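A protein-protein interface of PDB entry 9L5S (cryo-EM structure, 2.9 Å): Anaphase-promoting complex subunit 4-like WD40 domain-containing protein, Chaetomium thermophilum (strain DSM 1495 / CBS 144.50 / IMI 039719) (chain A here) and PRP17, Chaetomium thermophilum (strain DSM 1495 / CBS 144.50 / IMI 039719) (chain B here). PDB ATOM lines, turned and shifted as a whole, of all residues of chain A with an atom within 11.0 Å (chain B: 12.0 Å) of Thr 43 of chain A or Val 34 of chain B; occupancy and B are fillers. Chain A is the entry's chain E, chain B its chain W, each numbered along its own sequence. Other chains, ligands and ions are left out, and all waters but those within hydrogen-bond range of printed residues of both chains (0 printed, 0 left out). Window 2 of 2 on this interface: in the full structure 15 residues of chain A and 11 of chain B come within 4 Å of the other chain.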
ATOM      1  N   THR A  43      26.867   8.679  12.045  1.00  0.00           N
ATOM      2  CA  THR A  43      27.594   9.660  12.841  1.00  0.00           C
ATOM      3  C   THR A  43      28.927   9.111  13.332  1.00  0.00           C
ATOM      4  O   THR A  43      28.983   8.017  13.891  1.00  0.00           O
ATOM      5  CB  THR A  43      26.777  10.116  14.065  1.00  0.00           C
ATOM      6  OG1 THR A  43      26.320   8.970  14.794  1.00  0.00           O
ATOM      7  CG2 THR A  43      25.586  10.942  13.633  1.00  0.00           C
ATOM      8  N   PRO A  44      30.001   9.866  13.123  1.00  0.00           N
ATOM      9  CA  PRO A  44      31.290   9.502  13.715  1.00  0.00           C
ATOM     10  C   PRO A  44      31.335   9.884  15.188  1.00  0.00           C
ATOM     11  O   PRO A  44      30.465  10.585  15.707  1.00  0.00           O
ATOM     12  CB  PRO A  44      32.297  10.313  12.896  1.00  0.00           C
ATOM     13  CG  PRO A  44      31.533  11.515  12.465  1.00  0.00           C
ATOM     14  CD  PRO A  44      30.095  11.081  12.294  1.00  0.00           C
ATOM     15  N   ARG A  45      32.375   9.401  15.862  1.00  0.00           N
ATOM     16  CA  ARG A  45      32.530   9.670  17.285  1.00  0.00           C
ATOM     17  C   ARG A  45      32.909  11.129  17.508  1.00  0.00           C
ATOM     18  O   ARG A  45      33.797  11.662  16.835  1.00  0.00           O
ATOM     19  CB  ARG A  45      33.587   8.747  17.887  1.00  0.00           C
ATOM     20  CG  ARG A  45      33.785   8.934  19.380  1.00  0.00           C
ATOM     21  CD  ARG A  45      32.468   8.786  20.137  1.00  0.00           C
ATOM     22  NE  ARG A  45      31.847   7.487  19.906  1.00  0.00           N
ATOM     23  CZ  ARG A  45      32.176   6.372  20.544  1.00  0.00           C
ATOM     24  NH1 ARG A  45      33.105   6.362  21.487  1.00  0.00           N
ATOM     25  NH2 ARG A  45      31.557   5.239  20.229  1.00  0.00           N
ATOM     26  N   THR A  46      32.230  11.777  18.454  1.00  0.00           N
ATOM     27  CA  THR A  46      32.442  13.186  18.758  1.00  0.00           C
ATOM     28  C   THR A  46      33.196  13.401  20.064  1.00  0.00           C
ATOM     29  O   THR A  46      34.125  14.214  20.118  1.00  0.00           O
ATOM     30  CB  THR A  46      31.090  13.914  18.813  1.00  0.00           C
ATOM     31  OG1 THR A  46      30.402  13.742  17.566  1.00  0.00           O
ATOM     32  CG2 THR A  46      31.287  15.398  19.069  1.00  0.00           C
ATOM     33  N   SER A  47      32.835  12.675  21.114  1.00  0.00           N
ATOM     34  CA  SER A  47      33.407  12.857  22.440  1.00  0.00           C
ATOM     35  C   SER A  47      34.165  11.606  22.875  1.00  0.00           C
ATOM     36  O   SER A  47      34.291  10.628  22.134  1.00  0.00           O
ATOM     37  CB  SER A  47      32.311  13.199  23.444  1.00  0.00           C
ATOM     38  OG  SER A  47      31.551  12.042  23.745  1.00  0.00           O
ATOM     39  N   ALA A  51      30.336   4.769  24.545  1.00  0.00           N
ATOM     40  CA  ALA A  51      29.274   4.620  23.563  1.00  0.00           C
ATOM     41  C   ALA A  51      28.728   6.003  23.251  1.00  0.00           C
ATOM     42  O   ALA A  51      28.789   6.898  24.102  1.00  0.00           O
ATOM     43  CB  ALA A  51      28.161   3.700  24.082  1.00  0.00           C
ATOM     44  N   PRO A  52      28.198   6.217  22.039  1.00  0.00           N
ATOM     45  CA  PRO A  52      27.625   7.537  21.714  1.00  0.00           C
ATOM     46  C   PRO A  52      26.456   7.928  22.602  1.00  0.00           C
ATOM     47  O   PRO A  52      26.245   9.123  22.844  1.00  0.00           O
ATOM     48  CB  PRO A  52      27.190   7.381  20.248  1.00  0.00           C
ATOM     49  CG  PRO A  52      27.108   5.908  20.024  1.00  0.00           C
ATOM     50  CD  PRO A  52      28.191   5.325  20.868  1.00  0.00           C
ATOM     51  N   LEU A  53      25.698   6.953  23.094  1.00  0.00           N
ATOM     52  CA  LEU A  53      24.646   7.195  24.067  1.00  0.00           C
ATOM     53  C   LEU A  53      24.404   5.902  24.826  1.00  0.00           C
ATOM     54  O   LEU A  53      24.456   4.817  24.242  1.00  0.00           O
ATOM     55  CB  LEU A  53      23.364   7.694  23.397  1.00  0.00           C
ATOM     56  CG  LEU A  53      22.228   8.156  24.303  1.00  0.00           C
ATOM     57  CD1 LEU A  53      21.596   9.328  23.640  1.00  0.00           C
ATOM     58  CD2 LEU A  53      21.185   7.067  24.484  1.00  0.00           C
ATOM     59  N   ILE A 305      16.277  21.074  23.105  1.00  0.00           N
ATOM     60  CA  ILE A 305      17.451  21.933  23.156  1.00  0.00           C
ATOM     61  C   ILE A 305      17.240  23.057  22.156  1.00  0.00           C
ATOM     62  O   ILE A 305      17.025  22.800  20.965  1.00  0.00           O
ATOM     63  CB  ILE A 305      18.741  21.164  22.834  1.00  0.00           C
ATOM     64  CG1 ILE A 305      18.951  20.017  23.817  1.00  0.00           C
ATOM     65  CG2 ILE A 305      19.938  22.099  22.854  1.00  0.00           C
ATOM     66  CD1 ILE A 305      20.079  19.096  23.419  1.00  0.00           C
ATOM     67  N   LEU A 313      14.652  25.413  17.442  1.00  0.00           N
ATOM     68  CA  LEU A 313      14.619  24.123  18.124  1.00  0.00           C
ATOM     69  C   LEU A 313      15.790  23.310  17.586  1.00  0.00           C
ATOM     70  O   LEU A 313      15.703  22.708  16.517  1.00  0.00           O
ATOM     71  CB  LEU A 313      13.280  23.426  17.897  1.00  0.00           C
ATOM     72  CG  LEU A 313      12.899  22.181  18.711  1.00  0.00           C
ATOM     73  CD1 LEU A 313      11.391  22.123  18.869  1.00  0.00           C
ATOM     74  CD2 LEU A 313      13.390  20.886  18.074  1.00  0.00           C
ATOM     75  N   LEU A 314      16.904  23.313  18.320  1.00  0.00           N
ATOM     76  CA  LEU A 314      18.098  22.622  17.843  1.00  0.00           C
ATOM     77  C   LEU A 314      17.954  21.110  17.965  1.00  0.00           C
ATOM     78  O   LEU A 314      18.457  20.364  17.116  1.00  0.00           O
ATOM     79  CB  LEU A 314      19.330  23.108  18.609  1.00  0.00           C
ATOM     80  CG  LEU A 314      20.180  24.202  17.958  1.00  0.00           C
ATOM     81  CD1 LEU A 314      19.413  25.509  17.826  1.00  0.00           C
ATOM     82  CD2 LEU A 314      21.463  24.414  18.744  1.00  0.00           C
ATOM     83  N   TYR A 315      17.280  20.636  19.011  1.00  0.00           N
ATOM     84  CA  TYR A 315      17.151  19.204  19.239  1.00  0.00           C
ATOM     85  C   TYR A 315      15.831  18.904  19.930  1.00  0.00           C
ATOM     86  O   TYR A 315      15.356  19.689  20.752  1.00  0.00           O
ATOM     87  CB  TYR A 315      18.292  18.654  20.105  1.00  0.00           C
ATOM     88  CG  TYR A 315      19.631  18.547  19.418  1.00  0.00           C
ATOM     89  CD1 TYR A 315      19.969  17.417  18.686  1.00  0.00           C
ATOM     90  CD2 TYR A 315      20.568  19.566  19.522  1.00  0.00           C
ATOM     91  CE1 TYR A 315      21.198  17.313  18.064  1.00  0.00           C
ATOM     92  CE2 TYR A 315      21.797  19.473  18.903  1.00  0.00           C
ATOM     93  CZ  TYR A 315      22.107  18.344  18.176  1.00  0.00           C
ATOM     94  OH  TYR A 315      23.332  18.246  17.559  1.00  0.00           O
ATOM     95  N   LYS A 316      15.258  17.744  19.604  1.00  0.00           N
ATOM     96  CA  LYS A 316      14.177  17.142  20.392  1.00  0.00           C
ATOM     97  C   LYS A 316      14.532  15.664  20.531  1.00  0.00           C
ATOM     98  O   LYS A 316      14.265  14.861  19.634  1.00  0.00           O
ATOM     99  CB  LYS A 316      12.807  17.343  19.761  1.00  0.00           C
ATOM    100  CG  LYS A 316      11.676  17.015  20.720  1.00  0.00           C
ATOM    101  CD  LYS A 316      10.307  17.213  20.102  1.00  0.00           C
ATOM    102  CE  LYS A 316       9.225  16.658  21.017  1.00  0.00           C
ATOM    103  NZ  LYS A 316       7.887  16.620  20.366  1.00  0.00           N
ATOM    104  N   LEU A 317      15.131  15.315  21.669  1.00  0.00           N
ATOM    105  CA  LEU A 317      15.765  14.019  21.848  1.00  0.00           C
ATOM    106  C   LEU A 317      14.828  13.062  22.574  1.00  0.00           C
ATOM    107  O   LEU A 317      14.551  13.271  23.764  1.00  0.00           O
ATOM    108  CB  LEU A 317      17.058  14.180  22.627  1.00  0.00           C
ATOM    109  CG  LEU A 317      18.080  15.160  22.050  1.00  0.00           C
ATOM    110  CD1 LEU A 317      19.176  15.443  23.060  1.00  0.00           C
ATOM    111  CD2 LEU A 317      18.668  14.613  20.766  1.00  0.00           C
ATOM    112  N   PRO A 318      14.342  12.003  21.928  1.00  0.00           N
ATOM    113  CA  PRO A 318      13.495  11.030  22.627  1.00  0.00           C
ATOM    114  C   PRO A 318      14.308   9.992  23.384  1.00  0.00           C
ATOM    115  O   PRO A 318      15.528  10.121  23.508  1.00  0.00           O
ATOM    116  CB  PRO A 318      12.693  10.396  21.488  1.00  0.00           C
ATOM    117  CG  PRO A 318      13.630  10.444  20.331  1.00  0.00           C
ATOM    118  CD  PRO A 318      14.501  11.669  20.503  1.00  0.00           C
ATOM    119  N   GLY A 349      24.308  11.085  26.603  1.00  0.00           N
ATOM    120  CA  GLY A 349      24.459  11.169  25.170  1.00  0.00           C
ATOM    121  C   GLY A 349      25.461  12.238  24.785  1.00  0.00           C
ATOM    122  O   GLY A 349      25.776  13.140  25.561  1.00  0.00           O
ATOM    123  N   GLU A 350      25.963  12.115  23.562  1.00  0.00           N
ATOM    124  CA  GLU A 350      26.846  13.111  22.977  1.00  0.00           C
ATOM    125  C   GLU A 350      26.119  13.853  21.863  1.00  0.00           C
ATOM    126  O   GLU A 350      25.250  13.298  21.183  1.00  0.00           O
ATOM    127  CB  GLU A 350      28.138  12.469  22.452  1.00  0.00           C
ATOM    128  CG  GLU A 350      27.976  11.572  21.236  1.00  0.00           C
ATOM    129  CD  GLU A 350      29.256  10.842  20.882  1.00  0.00           C
ATOM    130  OE1 GLU A 350      30.260  11.022  21.603  1.00  0.00           O
ATOM    131  OE2 GLU A 350      29.260  10.091  19.885  1.00  0.00           O
ATOM    132  N   LEU A 351      26.461  15.128  21.701  1.00  0.00           N
ATOM    133  CA  LEU A 351      25.833  15.976  20.698  1.00  0.00           C
ATOM    134  C   LEU A 351      26.710  16.002  19.454  1.00  0.00           C
ATOM    135  O   LEU A 351      27.878  16.404  19.518  1.00  0.00           O
ATOM    136  CB  LEU A 351      25.615  17.386  21.244  1.00  0.00           C
ATOM    137  CG  LEU A 351      24.672  17.493  22.445  1.00  0.00           C
ATOM    138  CD1 LEU A 351      24.632  18.916  22.971  1.00  0.00           C
ATOM    139  CD2 LEU A 351      23.277  17.017  22.078  1.00  0.00           C
ATOM    140  N   ILE A 352      26.148  15.579  18.327  1.00  0.00           N
ATOM    141  CA  ILE A 352      26.912  15.443  17.094  1.00  0.00           C
ATOM    142  C   ILE A 352      26.438  16.459  16.061  1.00  0.00           C
ATOM    143  O   ILE A 352      27.242  17.113  15.397  1.00  0.00           O
ATOM    144  CB  ILE A 352      26.809  14.008  16.547  1.00  0.00           C
ATOM    145  CG1 ILE A 352      27.149  12.997  17.645  1.00  0.00           C
ATOM    146  CG2 ILE A 352      27.730  13.820  15.352  1.00  0.00           C
ATOM    147  CD1 ILE A 352      26.489  11.651  17.467  1.00  0.00           C
ATOM    148  OXT ILE A 352      25.238  16.657  15.873  1.00  0.00           O
ATOM    149  N   VAL B  34      21.190  14.261  14.523  1.00  0.00           N
ATOM    150  CA  VAL B  34      20.616  13.578  13.373  1.00  0.00           C
ATOM    151  C   VAL B  34      20.319  12.116  13.742  1.00  0.00           C
ATOM    152  O   VAL B  34      21.147  11.435  14.352  1.00  0.00           O
ATOM    153  CB  VAL B  34      21.545  13.737  12.117  1.00  0.00           C
ATOM    154  CG1 VAL B  34      22.894  13.062  12.305  1.00  0.00           C
ATOM    155  CG2 VAL B  34      20.870  13.216  10.856  1.00  0.00           C
ATOM    156  N   PRO B  35      19.094  11.646  13.446  1.00  0.00           N
ATOM    157  CA  PRO B  35      17.955  12.361  12.856  1.00  0.00           C
ATOM    158  C   PRO B  35      17.063  13.049  13.886  1.00  0.00           C
ATOM    159  O   PRO B  35      15.848  13.105  13.701  1.00  0.00           O
ATOM    160  CB  PRO B  35      17.189  11.249  12.147  1.00  0.00           C
ATOM    161  CG  PRO B  35      17.439  10.041  12.993  1.00  0.00           C
ATOM    162  CD  PRO B  35      18.770  10.229  13.689  1.00  0.00           C
ATOM    163  N   TYR B  36      17.661  13.558  14.959  1.00  0.00           N
ATOM    164  CA  TYR B  36      16.924  14.188  16.042  1.00  0.00           C
ATOM    165  C   TYR B  36      17.008  15.709  16.019  1.00  0.00           C
ATOM    166  O   TYR B  36      16.416  16.362  16.884  1.00  0.00           O
ATOM    167  CB  TYR B  36      17.430  13.661  17.387  1.00  0.00           C
ATOM    168  CG  TYR B  36      17.353  12.157  17.506  1.00  0.00           C
ATOM    169  CD1 TYR B  36      16.154  11.486  17.313  1.00  0.00           C
ATOM    170  CD2 TYR B  36      18.485  11.406  17.799  1.00  0.00           C
ATOM    171  CE1 TYR B  36      16.080  10.110  17.417  1.00  0.00           C
ATOM    172  CE2 TYR B  36      18.422  10.030  17.905  1.00  0.00           C
ATOM    173  CZ  TYR B  36      17.216   9.388  17.711  1.00  0.00           C
ATOM    174  OH  TYR B  36      17.147   8.019  17.816  1.00  0.00           O
ATOM    175  N   THR B  37      17.725  16.287  15.058  1.00  0.00           N
ATOM    176  CA  THR B  37      17.862  17.734  14.987  1.00  0.00           C
ATOM    177  C   THR B  37      16.574  18.382  14.489  1.00  0.00           C
ATOM    178  O   THR B  37      15.656  17.719  14.001  1.00  0.00           O
ATOM    179  CB  THR B  37      19.022  18.128  14.075  1.00  0.00           C
ATOM    180  OG1 THR B  37      18.737  17.717  12.733  1.00  0.00           O
ATOM    181  CG2 THR B  37      20.316  17.489  14.542  1.00  0.00           C
ATOM    182  N   GLY B  38      16.521  19.709  14.622  1.00  0.00           N
ATOM    183  CA  GLY B  38      15.312  20.442  14.285  1.00  0.00           C
ATOM    184  C   GLY B  38      14.984  20.459  12.807  1.00  0.00           C
ATOM    185  O   GLY B  38      13.811  20.397  12.433  1.00  0.00           O
ATOM    186  N   GLU B  39      16.001  20.556  11.947  1.00  0.00           N
ATOM    187  CA  GLU B  39      15.732  20.596  10.512  1.00  0.00           C
ATOM    188  C   GLU B  39      15.301  19.234   9.982  1.00  0.00           C
ATOM    189  O   GLU B  39      14.628  19.161   8.947  1.00  0.00           O
ATOM    190  CB  GLU B  39      16.957  21.118   9.752  1.00  0.00           C
ATOM    191  CG  GLU B  39      18.076  20.109   9.522  1.00  0.00           C
ATOM    192  CD  GLU B  39      19.075  20.057  10.666  1.00  0.00           C
ATOM    193  OE1 GLU B  39      18.749  20.524  11.777  1.00  0.00           O
ATOM    194  OE2 GLU B  39      20.193  19.544  10.451  1.00  0.00           O
ATOM    195  N   ASN B  40      15.672  18.150  10.667  1.00  0.00           N
ATOM    196  CA  ASN B  40      15.211  16.826  10.266  1.00  0.00           C
ATOM    197  C   ASN B  40      13.764  16.587  10.681  1.00  0.00           C
ATOM    198  O   ASN B  40      12.994  15.978   9.931  1.00  0.00           O
ATOM    199  CB  ASN B  40      16.125  15.755  10.860  1.00  0.00           C
ATOM    200  CG  ASN B  40      17.537  15.833  10.321  1.00  0.00           C
ATOM    201  OD1 ASN B  40      18.495  15.491  11.011  1.00  0.00           O
ATOM    202  ND2 ASN B  40      17.673  16.285   9.081  1.00  0.00           N
ATOM    203  N   LEU B  41      13.378  17.046  11.873  1.00  0.00           N
ATOM    204  CA  LEU B  41      11.985  16.943  12.291  1.00  0.00           C
ATOM    205  C   LEU B  41      11.095  17.956  11.585  1.00  0.00           C
ATOM    206  O   LEU B  41       9.879  17.749  11.512  1.00  0.00           O
ATOM    207  CB  LEU B  41      11.858  17.114  13.810  1.00  0.00           C
ATOM    208  CG  LEU B  41      12.089  15.931  14.764  1.00  0.00           C
ATOM    209  CD1 LEU B  41      11.040  14.852  14.524  1.00  0.00           C
ATOM    210  CD2 LEU B  41      13.495  15.342  14.698  1.00  0.00           C
ATOM    211  N   ALA B  42      11.667  19.041  11.068  1.00  0.00           N
ATOM    212  CA  ALA B  42      10.893  20.082  10.404  1.00  0.00           C
ATOM    213  C   ALA B  42      10.455  19.696   9.000  1.00  0.00           C
ATOM    214  O   ALA B  42       9.401  20.156   8.544  1.00  0.00           O
ATOM    215  CB  ALA B  42      11.700  21.381  10.345  1.00  0.00           C
ATOM    216  N   ARG B  43      11.237  18.881   8.300  1.00  0.00           N
ATOM    217  CA  ARG B  43      10.885  18.510   6.935  1.00  0.00           C
ATOM    218  C   ARG B  43       9.690  17.559   6.943  1.00  0.00           C
ATOM    219  O   ARG B  43       9.600  16.685   7.814  1.00  0.00           O
ATOM    220  CB  ARG B  43      12.093  17.892   6.216  1.00  0.00           C
ATOM    221  CG  ARG B  43      12.561  16.538   6.736  1.00  0.00           C
ATOM    222  CD  ARG B  43      13.766  16.014   5.968  1.00  0.00           C
ATOM    223  NE  ARG B  43      14.947  16.850   6.147  1.00  0.00           N
ATOM    224  CZ  ARG B  43      15.458  17.639   5.212  1.00  0.00           C
ATOM    225  NH1 ARG B  43      14.908  17.733   4.012  1.00  0.00           N
ATOM    226  NH2 ARG B  43      16.547  18.351   5.487  1.00  0.00           N
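Hydrophobic or aromatic side chains of chain B within 4 Å of the printed part of chain A: Val 34 and Tyr 36. Of the 19 printed residues of chain A, 7 touch a printed residue of chain B. Hydrophobic or aromatic side chains of chain A that line the printed part of chain B: Tyr 315, Leu 317 and Pro 318. Among the printed residues, 9 pairs touch across the chains. Among the printed residues, no Asp or Glu carboxylate lies within 4 Å of a Lys or Arg side-chain nitrogen of the other chain.
The side-chain hydroxyl (OG1) of Thr 37 of chain B sits at hydrogen-bond distance from the side-chain carboxylate (OE1) of Glu 39 of chain B (3.0 Å). The side-chain hydroxyl of Thr 37 of chain B sits at hydrogen-bond distance from the side-chain amide oxygen of Asn 40 of chain B, at 2.8 Å. N of Leu 314 of chain A sits at hydrogen-bond distance from O of Ile 305 of chain A, 2.7 Å away. The backbone carbonyl oxygen of Tyr 315 of chain A sits at hydrogen-bond distance from the backbone NH of Ile 305 of chain A (2.9 Å). OXT of Ile 352 of chain A lies within hydrogen-bond range of OH of Tyr 315 of chain A (3.0 Å).
Among the printed residues, pairs that only touch across the chains: Thr 43 of chain A with Val 34 of chain B, Leu 313 of chain A with Gly 38 of chain B, Leu 314 of chain A with Thr 37 of chain B, Tyr 315 of chain A with Tyr 36 of chain B, Tyr 315 of chain A with Thr 37 of chain B, Leu 317 of chain A with Tyr 36 of chain B and Pro 318 of chain A with Tyr 36 of chain B.
Thr 43 of chain A touches just one residue of chain B: Val 34. No residue of chain B comes within 4 Å of Pro 44 of chain A. Arg 45 of chain A touches none of the printed residues of chain B. Ile 305 of chain A touches none of the printed residues of chain B. Printed residues of chain B within 4 Å of Leu 314 of chain A: Thr 37 (3.4 Å) and Gly 38 (3.2 Å). Val 34 of chain B touches just one residue of chain A: Thr 43. Of chain A, only Tyr 315, Lys 316, Leu 317 and Pro 318 come within 4 Å of Tyr 36 of chain B. Thr 37 of chain B touches just these residues of chain A: Leu 314 (3.4 Å) and Tyr 315 (3.6 Å). Printed residues of chain A within 4 Å of Gly 38 of chain B: Leu 313 (3.2 Å) and Leu 314 (3.2 Å). The nearest residue of chain A that does not touch Val 34 of chain B is Tyr 315 of chain A (4.7 Å). The nearest printed residue of chain B that does not touch Leu 317 of chain A is Thr 37 of chain B (6.0 Å).
The backbone NH (N) of Lys 316 of chain A is in hydrogen-bond range of the backbone carbonyl oxygen (O) of Tyr 36 of chain B. The backbone NH of Gly 38 of chain B sits at hydrogen-bond distance from the backbone carbonyl oxygen of Leu 314 of chain A, 3.2 Å away.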
